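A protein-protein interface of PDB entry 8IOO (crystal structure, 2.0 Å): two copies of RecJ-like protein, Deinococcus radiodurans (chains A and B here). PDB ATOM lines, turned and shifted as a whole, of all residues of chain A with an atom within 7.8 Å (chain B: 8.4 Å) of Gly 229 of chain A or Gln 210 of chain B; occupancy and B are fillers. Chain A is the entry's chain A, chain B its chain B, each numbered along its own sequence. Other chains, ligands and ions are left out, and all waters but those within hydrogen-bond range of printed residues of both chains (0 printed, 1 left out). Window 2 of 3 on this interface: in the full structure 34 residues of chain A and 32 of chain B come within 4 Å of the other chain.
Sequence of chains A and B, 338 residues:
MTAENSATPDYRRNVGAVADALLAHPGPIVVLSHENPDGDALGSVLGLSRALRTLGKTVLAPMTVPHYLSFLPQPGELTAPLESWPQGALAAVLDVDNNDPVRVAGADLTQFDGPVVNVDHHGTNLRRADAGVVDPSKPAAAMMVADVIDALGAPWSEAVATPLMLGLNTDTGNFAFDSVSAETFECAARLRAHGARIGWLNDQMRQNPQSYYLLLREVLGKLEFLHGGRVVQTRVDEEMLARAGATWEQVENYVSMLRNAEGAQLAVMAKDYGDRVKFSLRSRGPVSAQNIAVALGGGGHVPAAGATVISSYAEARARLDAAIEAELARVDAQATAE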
ATOM      1  N   LEU A 223       7.716 -24.523  12.448  1.00  0.00           N
ATOM      2  CA  LEU A 223       8.293 -25.317  11.354  1.00  0.00           C
ATOM      3  C   LEU A 223       7.636 -26.698  11.238  1.00  0.00           C
ATOM      4  O   LEU A 223       7.187 -27.284  12.251  1.00  0.00           O
ATOM      5  CB  LEU A 223       9.767 -25.424  11.543  1.00  0.00           C
ATOM      6  CG  LEU A 223      10.590 -25.901  10.301  1.00  0.00           C
ATOM      7  CD1 LEU A 223      10.254 -25.029   9.137  1.00  0.00           C
ATOM      8  CD2 LEU A 223      12.052 -26.148  10.469  1.00  0.00           C
ATOM      9  N   GLU A 224       7.589 -27.243  10.008  1.00  0.00           N
ATOM     10  CA  GLU A 224       6.985 -28.529   9.808  1.00  0.00           C
ATOM     11  C   GLU A 224       7.646 -29.221   8.635  1.00  0.00           C
ATOM     12  O   GLU A 224       7.686 -28.677   7.519  1.00  0.00           O
ATOM     13  CB  GLU A 224       5.493 -28.339   9.537  1.00  0.00           C
ATOM     14  CG  GLU A 224       4.652 -28.090  10.791  1.00  0.00           C
ATOM     15  CD  GLU A 224       3.163 -28.087  10.469  1.00  0.00           C
ATOM     16  OE1 GLU A 224       2.656 -29.111   9.976  1.00  0.00           O
ATOM     17  OE2 GLU A 224       2.508 -27.021  10.637  1.00  0.00           O
ATOM     18  N   PHE A 225       8.071 -30.465   8.854  1.00  0.00           N
ATOM     19  CA  PHE A 225       8.511 -31.336   7.770  1.00  0.00           C
ATOM     20  C   PHE A 225       7.387 -32.312   7.439  1.00  0.00           C
ATOM     21  O   PHE A 225       6.921 -33.042   8.315  1.00  0.00           O
ATOM     22  CB  PHE A 225       9.789 -32.105   8.119  1.00  0.00           C
ATOM     23  CG  PHE A 225      11.007 -31.237   8.257  1.00  0.00           C
ATOM     24  CD1 PHE A 225      11.241 -30.528   9.422  1.00  0.00           C
ATOM     25  CD2 PHE A 225      11.849 -31.035   7.173  1.00  0.00           C
ATOM     26  CE1 PHE A 225      12.346 -29.706   9.547  1.00  0.00           C
ATOM     27  CE2 PHE A 225      12.942 -30.200   7.281  1.00  0.00           C
ATOM     28  CZ  PHE A 225      13.192 -29.528   8.468  1.00  0.00           C
ATOM     29  N   LEU A 226       6.977 -32.339   6.172  1.00  0.00           N
ATOM     30  CA  LEU A 226       5.827 -33.110   5.719  1.00  0.00           C
ATOM     31  C   LEU A 226       6.263 -33.913   4.510  1.00  0.00           C
ATOM     32  O   LEU A 226       7.302 -33.616   3.932  1.00  0.00           O
ATOM     33  CB  LEU A 226       4.657 -32.194   5.337  1.00  0.00           C
ATOM     34  CG  LEU A 226       4.378 -31.041   6.302  1.00  0.00           C
ATOM     35  CD1 LEU A 226       3.502 -29.972   5.651  1.00  0.00           C
ATOM     36  CD2 LEU A 226       3.734 -31.578   7.561  1.00  0.00           C
ATOM     37  N   HIS A 227       5.463 -34.919   4.118  1.00  0.00           N
ATOM     38  CA  HIS A 227       5.731 -35.805   2.961  1.00  0.00           C
ATOM     39  C   HIS A 227       7.127 -36.419   3.013  1.00  0.00           C
ATOM     40  O   HIS A 227       7.806 -36.541   1.985  1.00  0.00           O
ATOM     41  CB  HIS A 227       5.547 -35.081   1.619  1.00  0.00           C
ATOM     42  CG  HIS A 227       4.180 -34.512   1.412  1.00  0.00           C
ATOM     43  ND1 HIS A 227       3.150 -35.224   0.832  1.00  0.00           N
ATOM     44  CD2 HIS A 227       3.656 -33.314   1.765  1.00  0.00           C
ATOM     45  CE1 HIS A 227       2.062 -34.475   0.806  1.00  0.00           C
ATOM     46  NE2 HIS A 227       2.341 -33.314   1.370  1.00  0.00           N
ATOM     47  N   GLY A 228       7.576 -36.793   4.209  1.00  0.00           N
ATOM     48  CA  GLY A 228       8.866 -37.436   4.382  1.00  0.00           C
ATOM     49  C   GLY A 228      10.071 -36.565   4.100  1.00  0.00           C
ATOM     50  O   GLY A 228      11.017 -37.024   3.443  1.00  0.00           O
ATOM     51  N   GLY A 229      10.064 -35.319   4.572  1.00  0.00           N
ATOM     52  CA  GLY A 229      11.161 -34.403   4.358  1.00  0.00           C
ATOM     53  C   GLY A 229      11.133 -33.638   3.042  1.00  0.00           C
ATOM     54  O   GLY A 229      11.858 -32.643   2.909  1.00  0.00           O
ATOM     55  N   ARG A 230      10.321 -34.064   2.072  1.00  0.00           N
ATOM     56  CA  ARG A 230      10.260 -33.403   0.768  1.00  0.00           C
ATOM     57  C   ARG A 230       9.691 -31.988   0.850  1.00  0.00           C
ATOM     58  O   ARG A 230       9.986 -31.172  -0.028  1.00  0.00           O
ATOM     59  CB  ARG A 230       9.399 -34.238  -0.177  1.00  0.00           C
ATOM     60  CG  ARG A 230      10.038 -35.527  -0.612  1.00  0.00           C
ATOM     61  CD  ARG A 230       9.629 -35.876  -2.033  1.00  0.00           C
ATOM     62  NE  ARG A 230       8.333 -36.548  -2.071  1.00  0.00           N
ATOM     63  CZ  ARG A 230       7.695 -36.865  -3.184  1.00  0.00           C
ATOM     64  NH1 ARG A 230       8.191 -36.554  -4.369  1.00  0.00           N
ATOM     65  NH2 ARG A 230       6.536 -37.513  -3.105  1.00  0.00           N
ATOM     66  N   VAL A 231       8.875 -31.700   1.865  1.00  0.00           N
ATOM     67  CA  VAL A 231       8.127 -30.451   1.985  1.00  0.00           C
ATOM     68  C   VAL A 231       8.410 -29.857   3.350  1.00  0.00           C
ATOM     69  O   VAL A 231       8.084 -30.470   4.372  1.00  0.00           O
ATOM     70  CB  VAL A 231       6.610 -30.661   1.814  1.00  0.00           C
ATOM     71  CG1 VAL A 231       5.856 -29.383   2.156  1.00  0.00           C
ATOM     72  CG2 VAL A 231       6.282 -31.124   0.419  1.00  0.00           C
ATOM     73  N   VAL A 232       8.959 -28.649   3.372  1.00  0.00           N
ATOM     74  CA  VAL A 232       9.153 -27.919   4.617  1.00  0.00           C
ATOM     75  C   VAL A 232       8.310 -26.657   4.550  1.00  0.00           C
ATOM     76  O   VAL A 232       8.187 -26.025   3.496  1.00  0.00           O
ATOM     77  CB  VAL A 232      10.641 -27.587   4.872  1.00  0.00           C
ATOM     78  CG1 VAL A 232      11.288 -27.020   3.603  1.00  0.00           C
ATOM     79  CG2 VAL A 232      10.792 -26.615   6.034  1.00  0.00           C
ATOM     80  N   ASN A 260      17.170 -24.481   2.300  1.00  0.00           N
ATOM     81  CA  ASN A 260      18.447 -25.175   2.621  1.00  0.00           C
ATOM     82  C   ASN A 260      18.211 -26.555   3.258  1.00  0.00           C
ATOM     83  O   ASN A 260      19.194 -27.292   3.383  1.00  0.00           O
ATOM     84  CB  ASN A 260      19.309 -24.282   3.514  1.00  0.00           C
ATOM     85  CG  ASN A 260      19.797 -23.031   2.815  1.00  0.00           C
ATOM     86  OD1 ASN A 260      19.955 -23.014   1.598  1.00  0.00           O
ATOM     87  ND2 ASN A 260      20.045 -21.980   3.577  1.00  0.00           N
ATOM     88  N   ALA A 261      16.972 -26.905   3.619  1.00  0.00           N
ATOM     89  CA  ALA A 261      16.663 -28.167   4.285  1.00  0.00           C
ATOM     90  C   ALA A 261      16.969 -29.338   3.363  1.00  0.00           C
ATOM     91  O   ALA A 261      16.564 -29.355   2.195  1.00  0.00           O
ATOM     92  CB  ALA A 261      15.194 -28.201   4.711  1.00  0.00           C
ATOM     93  N   GLU A 262      17.682 -30.320   3.894  1.00  0.00           N
ATOM     94  CA  GLU A 262      18.217 -31.396   3.083  1.00  0.00           C
ATOM     95  C   GLU A 262      17.125 -32.434   2.828  1.00  0.00           C
ATOM     96  O   GLU A 262      16.384 -32.811   3.744  1.00  0.00           O
ATOM     97  CB  GLU A 262      19.425 -31.990   3.807  1.00  0.00           C
ATOM     98  CG  GLU A 262      20.335 -32.899   3.029  1.00  0.00           C
ATOM     99  CD  GLU A 262      21.409 -33.478   3.933  1.00  0.00           C
ATOM    100  OE1 GLU A 262      21.887 -32.744   4.826  1.00  0.00           O
ATOM    101  OE2 GLU A 262      21.764 -34.664   3.749  1.00  0.00           O
ATOM    102  N   GLY A 263      17.008 -32.876   1.579  1.00  0.00           N
ATOM    103  CA  GLY A 263      15.909 -33.703   1.139  1.00  0.00           C
ATOM    104  C   GLY A 263      14.672 -32.930   0.713  1.00  0.00           C
ATOM    105  O   GLY A 263      13.793 -33.510   0.063  1.00  0.00           O
ATOM    106  N   ALA A 264      14.572 -31.644   1.064  1.00  0.00           N
ATOM    107  CA  ALA A 264      13.380 -30.880   0.712  1.00  0.00           C
ATOM    108  C   ALA A 264      13.403 -30.481  -0.759  1.00  0.00           C
ATOM    109  O   ALA A 264      14.402 -29.953  -1.260  1.00  0.00           O
ATOM    110  CB  ALA A 264      13.261 -29.633   1.591  1.00  0.00           C
ATOM    111  N   GLN A 265      12.294 -30.732  -1.450  1.00  0.00           N
ATOM    112  CA  GLN A 265      12.096 -30.242  -2.809  1.00  0.00           C
ATOM    113  C   GLN A 265      11.146 -29.050  -2.871  1.00  0.00           C
ATOM    114  O   GLN A 265      10.875 -28.538  -3.963  1.00  0.00           O
ATOM    115  CB  GLN A 265      11.558 -31.359  -3.703  1.00  0.00           C
ATOM    116  CG  GLN A 265      12.560 -32.488  -3.899  1.00  0.00           C
ATOM    117  CD  GLN A 265      12.073 -33.572  -4.834  1.00  0.00           C
ATOM    118  OE1 GLN A 265      12.736 -33.917  -5.811  1.00  0.00           O
ATOM    119  NE2 GLN A 265      10.863 -34.051  -4.587  1.00  0.00           N
ATOM    120  N   LEU A 266      10.632 -28.608  -1.727  1.00  0.00           N
ATOM    121  CA  LEU A 266       9.678 -27.502  -1.641  1.00  0.00           C
ATOM    122  C   LEU A 266       9.785 -26.864  -0.271  1.00  0.00           C
ATOM    123  O   LEU A 266       9.686 -27.568   0.743  1.00  0.00           O
ATOM    124  CB  LEU A 266       8.251 -27.974  -1.884  1.00  0.00           C
ATOM    125  CG  LEU A 266       7.240 -26.830  -2.011  1.00  0.00           C
ATOM    126  CD1 LEU A 266       7.169 -26.304  -3.422  1.00  0.00           C
ATOM    127  CD2 LEU A 266       5.881 -27.327  -1.540  1.00  0.00           C
ATOM    128  N   GLN B 207      23.391 -26.446   2.725  1.00  0.00           N
ATOM    129  CA  GLN B 207      22.421 -27.519   3.080  1.00  0.00           C
ATOM    130  C   GLN B 207      22.487 -27.827   4.588  1.00  0.00           C
ATOM    131  O   GLN B 207      23.605 -27.892   5.112  1.00  0.00           O
ATOM    132  CB  GLN B 207      22.671 -28.770   2.243  1.00  0.00           C
ATOM    133  CG  GLN B 207      22.609 -28.531   0.746  1.00  0.00           C
ATOM    134  CD  GLN B 207      21.191 -28.299   0.293  1.00  0.00           C
ATOM    135  OE1 GLN B 207      20.492 -29.222  -0.112  1.00  0.00           O
ATOM    136  NE2 GLN B 207      20.758 -27.052   0.355  1.00  0.00           N
ATOM    137  N   ASN B 208      21.333 -28.006   5.250  1.00  0.00           N
ATOM    138  CA  ASN B 208      21.260 -28.352   6.699  1.00  0.00           C
ATOM    139  C   ASN B 208      20.249 -29.489   6.953  1.00  0.00           C
ATOM    140  O   ASN B 208      19.186 -29.470   6.318  1.00  0.00           O
ATOM    141  CB  ASN B 208      20.925 -27.143   7.576  1.00  0.00           C
ATOM    142  CG  ASN B 208      21.623 -25.857   7.195  1.00  0.00           C
ATOM    143  OD1 ASN B 208      22.840 -25.749   7.306  1.00  0.00           O
ATOM    144  ND2 ASN B 208      20.854 -24.867   6.774  1.00  0.00           N
ATOM    145  N   PRO B 209      20.530 -30.478   7.846  1.00  0.00           N
ATOM    146  CA  PRO B 209      19.619 -31.600   8.077  1.00  0.00           C
ATOM    147  C   PRO B 209      18.460 -31.093   8.904  1.00  0.00           C
ATOM    148  O   PRO B 209      18.498 -29.992   9.451  1.00  0.00           O
ATOM    149  CB  PRO B 209      20.491 -32.624   8.804  1.00  0.00           C
ATOM    150  CG  PRO B 209      21.544 -31.808   9.471  1.00  0.00           C
ATOM    151  CD  PRO B 209      21.833 -30.686   8.481  1.00  0.00           C
ATOM    152  N   GLN B 210      17.385 -31.869   8.921  1.00  0.00           N
ATOM    153  CA  GLN B 210      16.269 -31.506   9.784  1.00  0.00           C
ATOM    154  C   GLN B 210      16.736 -31.359  11.221  1.00  0.00           C
ATOM    155  O   GLN B 210      16.234 -30.498  11.960  1.00  0.00           O
ATOM    156  CB  GLN B 210      15.163 -32.558   9.690  1.00  0.00           C
ATOM    157  CG  GLN B 210      14.791 -32.947   8.277  1.00  0.00           C
ATOM    158  CD  GLN B 210      13.477 -33.698   8.230  1.00  0.00           C
ATOM    159  OE1 GLN B 210      12.983 -34.046   7.156  1.00  0.00           O
ATOM    160  NE2 GLN B 210      12.884 -33.925   9.402  1.00  0.00           N
ATOM    161  N   SER B 211      17.712 -32.188  11.626  1.00  0.00           N
ATOM    162  CA  SER B 211      18.292 -32.099  12.966  1.00  0.00           C
ATOM    163  C   SER B 211      18.666 -30.666  13.316  1.00  0.00           C
ATOM    164  O   SER B 211      18.370 -30.180  14.415  1.00  0.00           O
ATOM    165  CB  SER B 211      19.525 -33.008  13.058  1.00  0.00           C
ATOM    166  OG  SER B 211      19.395 -34.116  12.188  1.00  0.00           O
ATOM    167  N   TYR B 212      19.300 -29.967  12.369  1.00  0.00           N
ATOM    168  CA  TYR B 212      19.772 -28.607  12.613  1.00  0.00           C
ATOM    169  C   TYR B 212      18.640 -27.677  13.017  1.00  0.00           C
ATOM    170  O   TYR B 212      18.786 -26.872  13.946  1.00  0.00           O
ATOM    171  CB  TYR B 212      20.477 -28.072  11.369  1.00  0.00           C
ATOM    172  CG  TYR B 212      20.674 -26.569  11.381  1.00  0.00           C
ATOM    173  CD1 TYR B 212      21.739 -25.991  12.058  1.00  0.00           C
ATOM    174  CD2 TYR B 212      19.797 -25.727  10.701  1.00  0.00           C
ATOM    175  CE1 TYR B 212      21.919 -24.614  12.051  1.00  0.00           C
ATOM    176  CE2 TYR B 212      19.976 -24.357  10.683  1.00  0.00           C
ATOM    177  CZ  TYR B 212      21.038 -23.799  11.363  1.00  0.00           C
ATOM    178  OH  TYR B 212      21.221 -22.430  11.362  1.00  0.00           O
ATOM    179  N   TYR B 213      17.507 -27.752  12.317  1.00  0.00           N
ATOM    180  CA  TYR B 213      16.431 -26.812  12.606  1.00  0.00           C
ATOM    181  C   TYR B 213      15.747 -27.169  13.919  1.00  0.00           C
ATOM    182  O   TYR B 213      15.502 -26.300  14.764  1.00  0.00           O
ATOM    183  CB  TYR B 213      15.412 -26.811  11.471  1.00  0.00           C
ATOM    184  CG  TYR B 213      15.991 -26.469  10.117  1.00  0.00           C
ATOM    185  CD1 TYR B 213      16.075 -25.150   9.678  1.00  0.00           C
ATOM    186  CD2 TYR B 213      16.442 -27.472   9.268  1.00  0.00           C
ATOM    187  CE1 TYR B 213      16.603 -24.848   8.439  1.00  0.00           C
ATOM    188  CE2 TYR B 213      16.966 -27.180   8.036  1.00  0.00           C
ATOM    189  CZ  TYR B 213      17.047 -25.868   7.622  1.00  0.00           C
ATOM    190  OH  TYR B 213      17.569 -25.581   6.382  1.00  0.00           O
ATOM    191  N   LEU B 214      15.450 -28.455  14.101  1.00  0.00           N
ATOM    192  CA  LEU B 214      14.780 -28.925  15.304  1.00  0.00           C
ATOM    193  C   LEU B 214      15.624 -28.637  16.539  1.00  0.00           C
ATOM    194  O   LEU B 214      15.100 -28.249  17.592  1.00  0.00           O
ATOM    195  CB  LEU B 214      14.523 -30.426  15.163  1.00  0.00           C
ATOM    196  CG  LEU B 214      13.500 -30.792  14.083  1.00  0.00           C
ATOM    197  CD1 LEU B 214      13.220 -32.284  14.072  1.00  0.00           C
ATOM    198  CD2 LEU B 214      12.214 -29.994  14.181  1.00  0.00           C
ATOM    199  N   LEU B 215      16.945 -28.810  16.420  1.00  0.00           N
ATOM    200  CA  LEU B 215      17.842 -28.541  17.538  1.00  0.00           C
ATOM    201  C   LEU B 215      17.988 -27.046  17.778  1.00  0.00           C
ATOM    202  O   LEU B 215      18.152 -26.617  18.927  1.00  0.00           O
ATOM    203  CB  LEU B 215      19.209 -29.175  17.272  1.00  0.00           C
ATOM    204  CG  LEU B 215      20.397 -28.962  18.222  1.00  0.00           C
ATOM    205  CD1 LEU B 215      19.983 -29.157  19.678  1.00  0.00           C
ATOM    206  CD2 LEU B 215      21.551 -29.884  17.850  1.00  0.00           C
ATOM    207  N   LEU B 216      17.926 -26.239  16.714  1.00  0.00           N
ATOM    208  CA  LEU B 216      18.001 -24.795  16.881  1.00  0.00           C
ATOM    209  C   LEU B 216      16.717 -24.236  17.482  1.00  0.00           C
ATOM    210  O   LEU B 216      16.757 -23.197  18.151  1.00  0.00           O
ATOM    211  CB  LEU B 216      18.311 -24.120  15.537  1.00  0.00           C
ATOM    212  CG  LEU B 216      18.203 -22.597  15.368  1.00  0.00           C
ATOM    213  CD1 LEU B 216      19.353 -21.868  16.045  1.00  0.00           C
ATOM    214  CD2 LEU B 216      18.147 -22.242  13.886  1.00  0.00           C
ATOM    215  N   ARG B 217      15.580 -24.908  17.269  1.00  0.00           N
ATOM    216  CA  ARG B 217      14.374 -24.552  18.009  1.00  0.00           C
ATOM    217  C   ARG B 217      14.571 -24.786  19.503  1.00  0.00           C
ATOM    218  O   ARG B 217      14.147 -23.968  20.329  1.00  0.00           O
ATOM    219  CB  ARG B 217      13.173 -25.356  17.495  1.00  0.00           C
ATOM    220  CG  ARG B 217      11.826 -24.833  17.985  1.00  0.00           C
ATOM    221  CD  ARG B 217      10.647 -25.795  17.746  1.00  0.00           C
ATOM    222  NE  ARG B 217      10.960 -27.220  17.718  1.00  0.00           N
ATOM    223  CZ  ARG B 217      10.184 -28.137  17.152  1.00  0.00           C
ATOM    224  NH1 ARG B 217       9.096 -27.802  16.479  1.00  0.00           N
ATOM    225  NH2 ARG B 217      10.505 -29.423  17.269  1.00  0.00           N
ATOM    226  N   ARG B 243      14.797 -35.124  21.194  1.00  0.00           N
ATOM    227  CA  ARG B 243      13.611 -34.599  20.532  1.00  0.00           C
ATOM    228  C   ARG B 243      13.946 -33.985  19.182  1.00  0.00           C
ATOM    229  O   ARG B 243      13.110 -34.004  18.272  1.00  0.00           O
ATOM    230  CB  ARG B 243      12.916 -33.570  21.426  1.00  0.00           C
ATOM    231  CG  ARG B 243      12.087 -34.245  22.496  1.00  0.00           C
ATOM    232  CD  ARG B 243      10.980 -33.386  23.109  1.00  0.00           C
ATOM    233  NE  ARG B 243      11.325 -32.032  23.539  1.00  0.00           N
ATOM    234  CZ  ARG B 243      12.248 -31.711  24.438  1.00  0.00           C
ATOM    235  NH1 ARG B 243      13.133 -32.592  24.879  1.00  0.00           N
ATOM    236  NH2 ARG B 243      12.295 -30.462  24.897  1.00  0.00           N
ATOM    237  N   ALA B 244      15.158 -33.454  19.027  1.00  0.00           N
ATOM    238  CA  ALA B 244      15.556 -32.910  17.735  1.00  0.00           C
ATOM    239  C   ALA B 244      16.022 -33.993  16.776  1.00  0.00           C
ATOM    240  O   ALA B 244      15.983 -33.789  15.562  1.00  0.00           O
ATOM    241  CB  ALA B 244      16.679 -31.885  17.905  1.00  0.00           C
ATOM    242  N   GLY B 245      16.465 -35.134  17.294  1.00  0.00           N
ATOM    243  CA  GLY B 245      17.081 -36.131  16.444  1.00  0.00           C
ATOM    244  C   GLY B 245      18.510 -35.813  16.078  1.00  0.00           C
ATOM    245  O   GLY B 245      18.992 -36.257  15.034  1.00  0.00           O
ATOM    246  N   ALA B 246      19.237 -35.151  16.981  1.00  0.00           N
ATOM    247  CA  ALA B 246      20.626 -34.731  16.676  1.00  0.00           C
ATOM    248  C   ALA B 246      21.667 -35.361  17.614  1.00  0.00           C
ATOM    249  O   ALA B 246      21.285 -36.167  18.478  1.00  0.00           O
ATOM    250  CB  ALA B 246      20.709 -33.233  16.752  1.00  0.00           C
ATOM    251  N   GLN B 250      26.782 -31.535  17.178  1.00  0.00           N
ATOM    252  CA  GLN B 250      25.999 -30.586  16.346  1.00  0.00           C
ATOM    253  C   GLN B 250      25.717 -29.353  17.205  1.00  0.00           C
ATOM    254  O   GLN B 250      25.378 -28.309  16.633  1.00  0.00           O
ATOM    255  CB  GLN B 250      24.728 -31.267  15.835  1.00  0.00           C
ATOM    256  CG  GLN B 250      24.848 -31.778  14.409  1.00  0.00           C
ATOM    257  CD  GLN B 250      23.716 -32.695  14.016  1.00  0.00           C
ATOM    258  OE1 GLN B 250      23.219 -33.480  14.819  1.00  0.00           O
ATOM    259  NE2 GLN B 250      23.303 -32.609  12.763  1.00  0.00           N
ATOM    260  N   TYR B 254      26.140 -23.415  17.251  1.00  0.00           N
ATOM    261  CA  TYR B 254      25.153 -22.427  17.759  1.00  0.00           C
ATOM    262  C   TYR B 254      25.824 -21.370  18.644  1.00  0.00           C
ATOM    263  O   TYR B 254      25.179 -20.345  18.912  1.00  0.00           O
ATOM    264  CB  TYR B 254      24.022 -23.162  18.485  1.00  0.00           C
ATOM    265  CG  TYR B 254      23.315 -24.186  17.637  1.00  0.00           C
ATOM    266  CD1 TYR B 254      22.500 -23.802  16.587  1.00  0.00           C
ATOM    267  CD2 TYR B 254      23.478 -25.540  17.869  1.00  0.00           C
ATOM    268  CE1 TYR B 254      21.856 -24.736  15.794  1.00  0.00           C
ATOM    269  CE2 TYR B 254      22.839 -26.485  17.088  1.00  0.00           C
ATOM    270  CZ  TYR B 254      22.024 -26.084  16.047  1.00  0.00           C
ATOM    271  OH  TYR B 254      21.391 -27.011  15.274  1.00  0.00           O
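CB of Tyr 213 of chain B touches CD2 of Leu 223 of chain A (3.6 Å).
Gln 210 of chain B touches Phe 225 of chain A (OE1 to CD2, 3.2 Å).
CD2 of Tyr 213 of chain B touches CZ of Phe 225 of chain A, 3.9 Å away.
OE1 of Gln 210 of chain B touches CA of Gly 229 of chain A (3.4 Å).
Asn 260 of chain A touches Tyr 213 of chain B (C to OH, 3.3 Å).
Asn 208 of chain B touches Ala 261 of chain A.
O of Gly 229 of chain A sits close to N of Ala 264 of chain A, at 3.4 Å.
OH of Tyr 213 of chain B sits at hydrogen-bond distance from ND2 of Asn 208 of chain B.
NE2 of Gln 207 of chain B lies close to O of Asn 260 of chain A.
The backbone carbonyl oxygen (O) of Asn 260 of chain A sits at hydrogen-bond distance from the backbone NH (N) of Asn 208 of chain B, 2.9 Å away.
N of Ala 261 of chain A is in hydrogen-bond range of OH of Tyr 213 of chain B (3.1 Å).
O of Asn 208 of chain B sits at hydrogen-bond distance from N of Glu 262 of chain A (3.0 Å).
Printed residues of chain B that touch a printed residue of chain A: Gln 207, Asn 208, Gln 210 and Tyr 213.
Printed residues of chain A that touch a printed residue of chain B: Leu 223, Phe 225, Gly 229, Asn 260, Ala 261 and Glu 262.
Hydrophobic or aromatic side chains of chain A that line the printed part of chain B: Leu 223, Phe 225 and Ala 261.
Along chain A the printed residues that touch a printed residue of chain B span positions 223 to 262.
Among the printed residues, no Asp or Glu carboxylate lies within 4 Å of a Lys or Arg side-chain nitrogen of the other chain.
No position is printed for both chains.
Of the 10 pairs that touch across the chains among the printed residues, none has its exchanged pair printed and touching as well.
Of chain B, only Gln 210 (3.4 Å) comes within 4 Å of Gly 229 of chain A.
Of chain A, only Phe 225 (3.2 Å) and Gly 229 (3.4 Å) come within 4 Å of Gln 210 of chain B.
No residue of chain B comes within 4 Å of Gly 228 of chain A.
Of the printed residues of chain B, Asn 260 of chain A touches Gln 207, Asn 208 and Tyr 213.
Of the printed residues of chain B, Phe 225 of chain A touches Gln 210 (3.2 Å) and Tyr 213 (3.9 Å).
Of the printed residues of chain A, Gln 207 of chain B touches Asn 260.
Of the printed residues of chain A, Asn 208 of chain B touches Asn 260, Ala 261 and Glu 262.
The nearest printed residue of chain B that does not touch Leu 223 of chain A is Arg 217 of chain B (4.7 Å).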
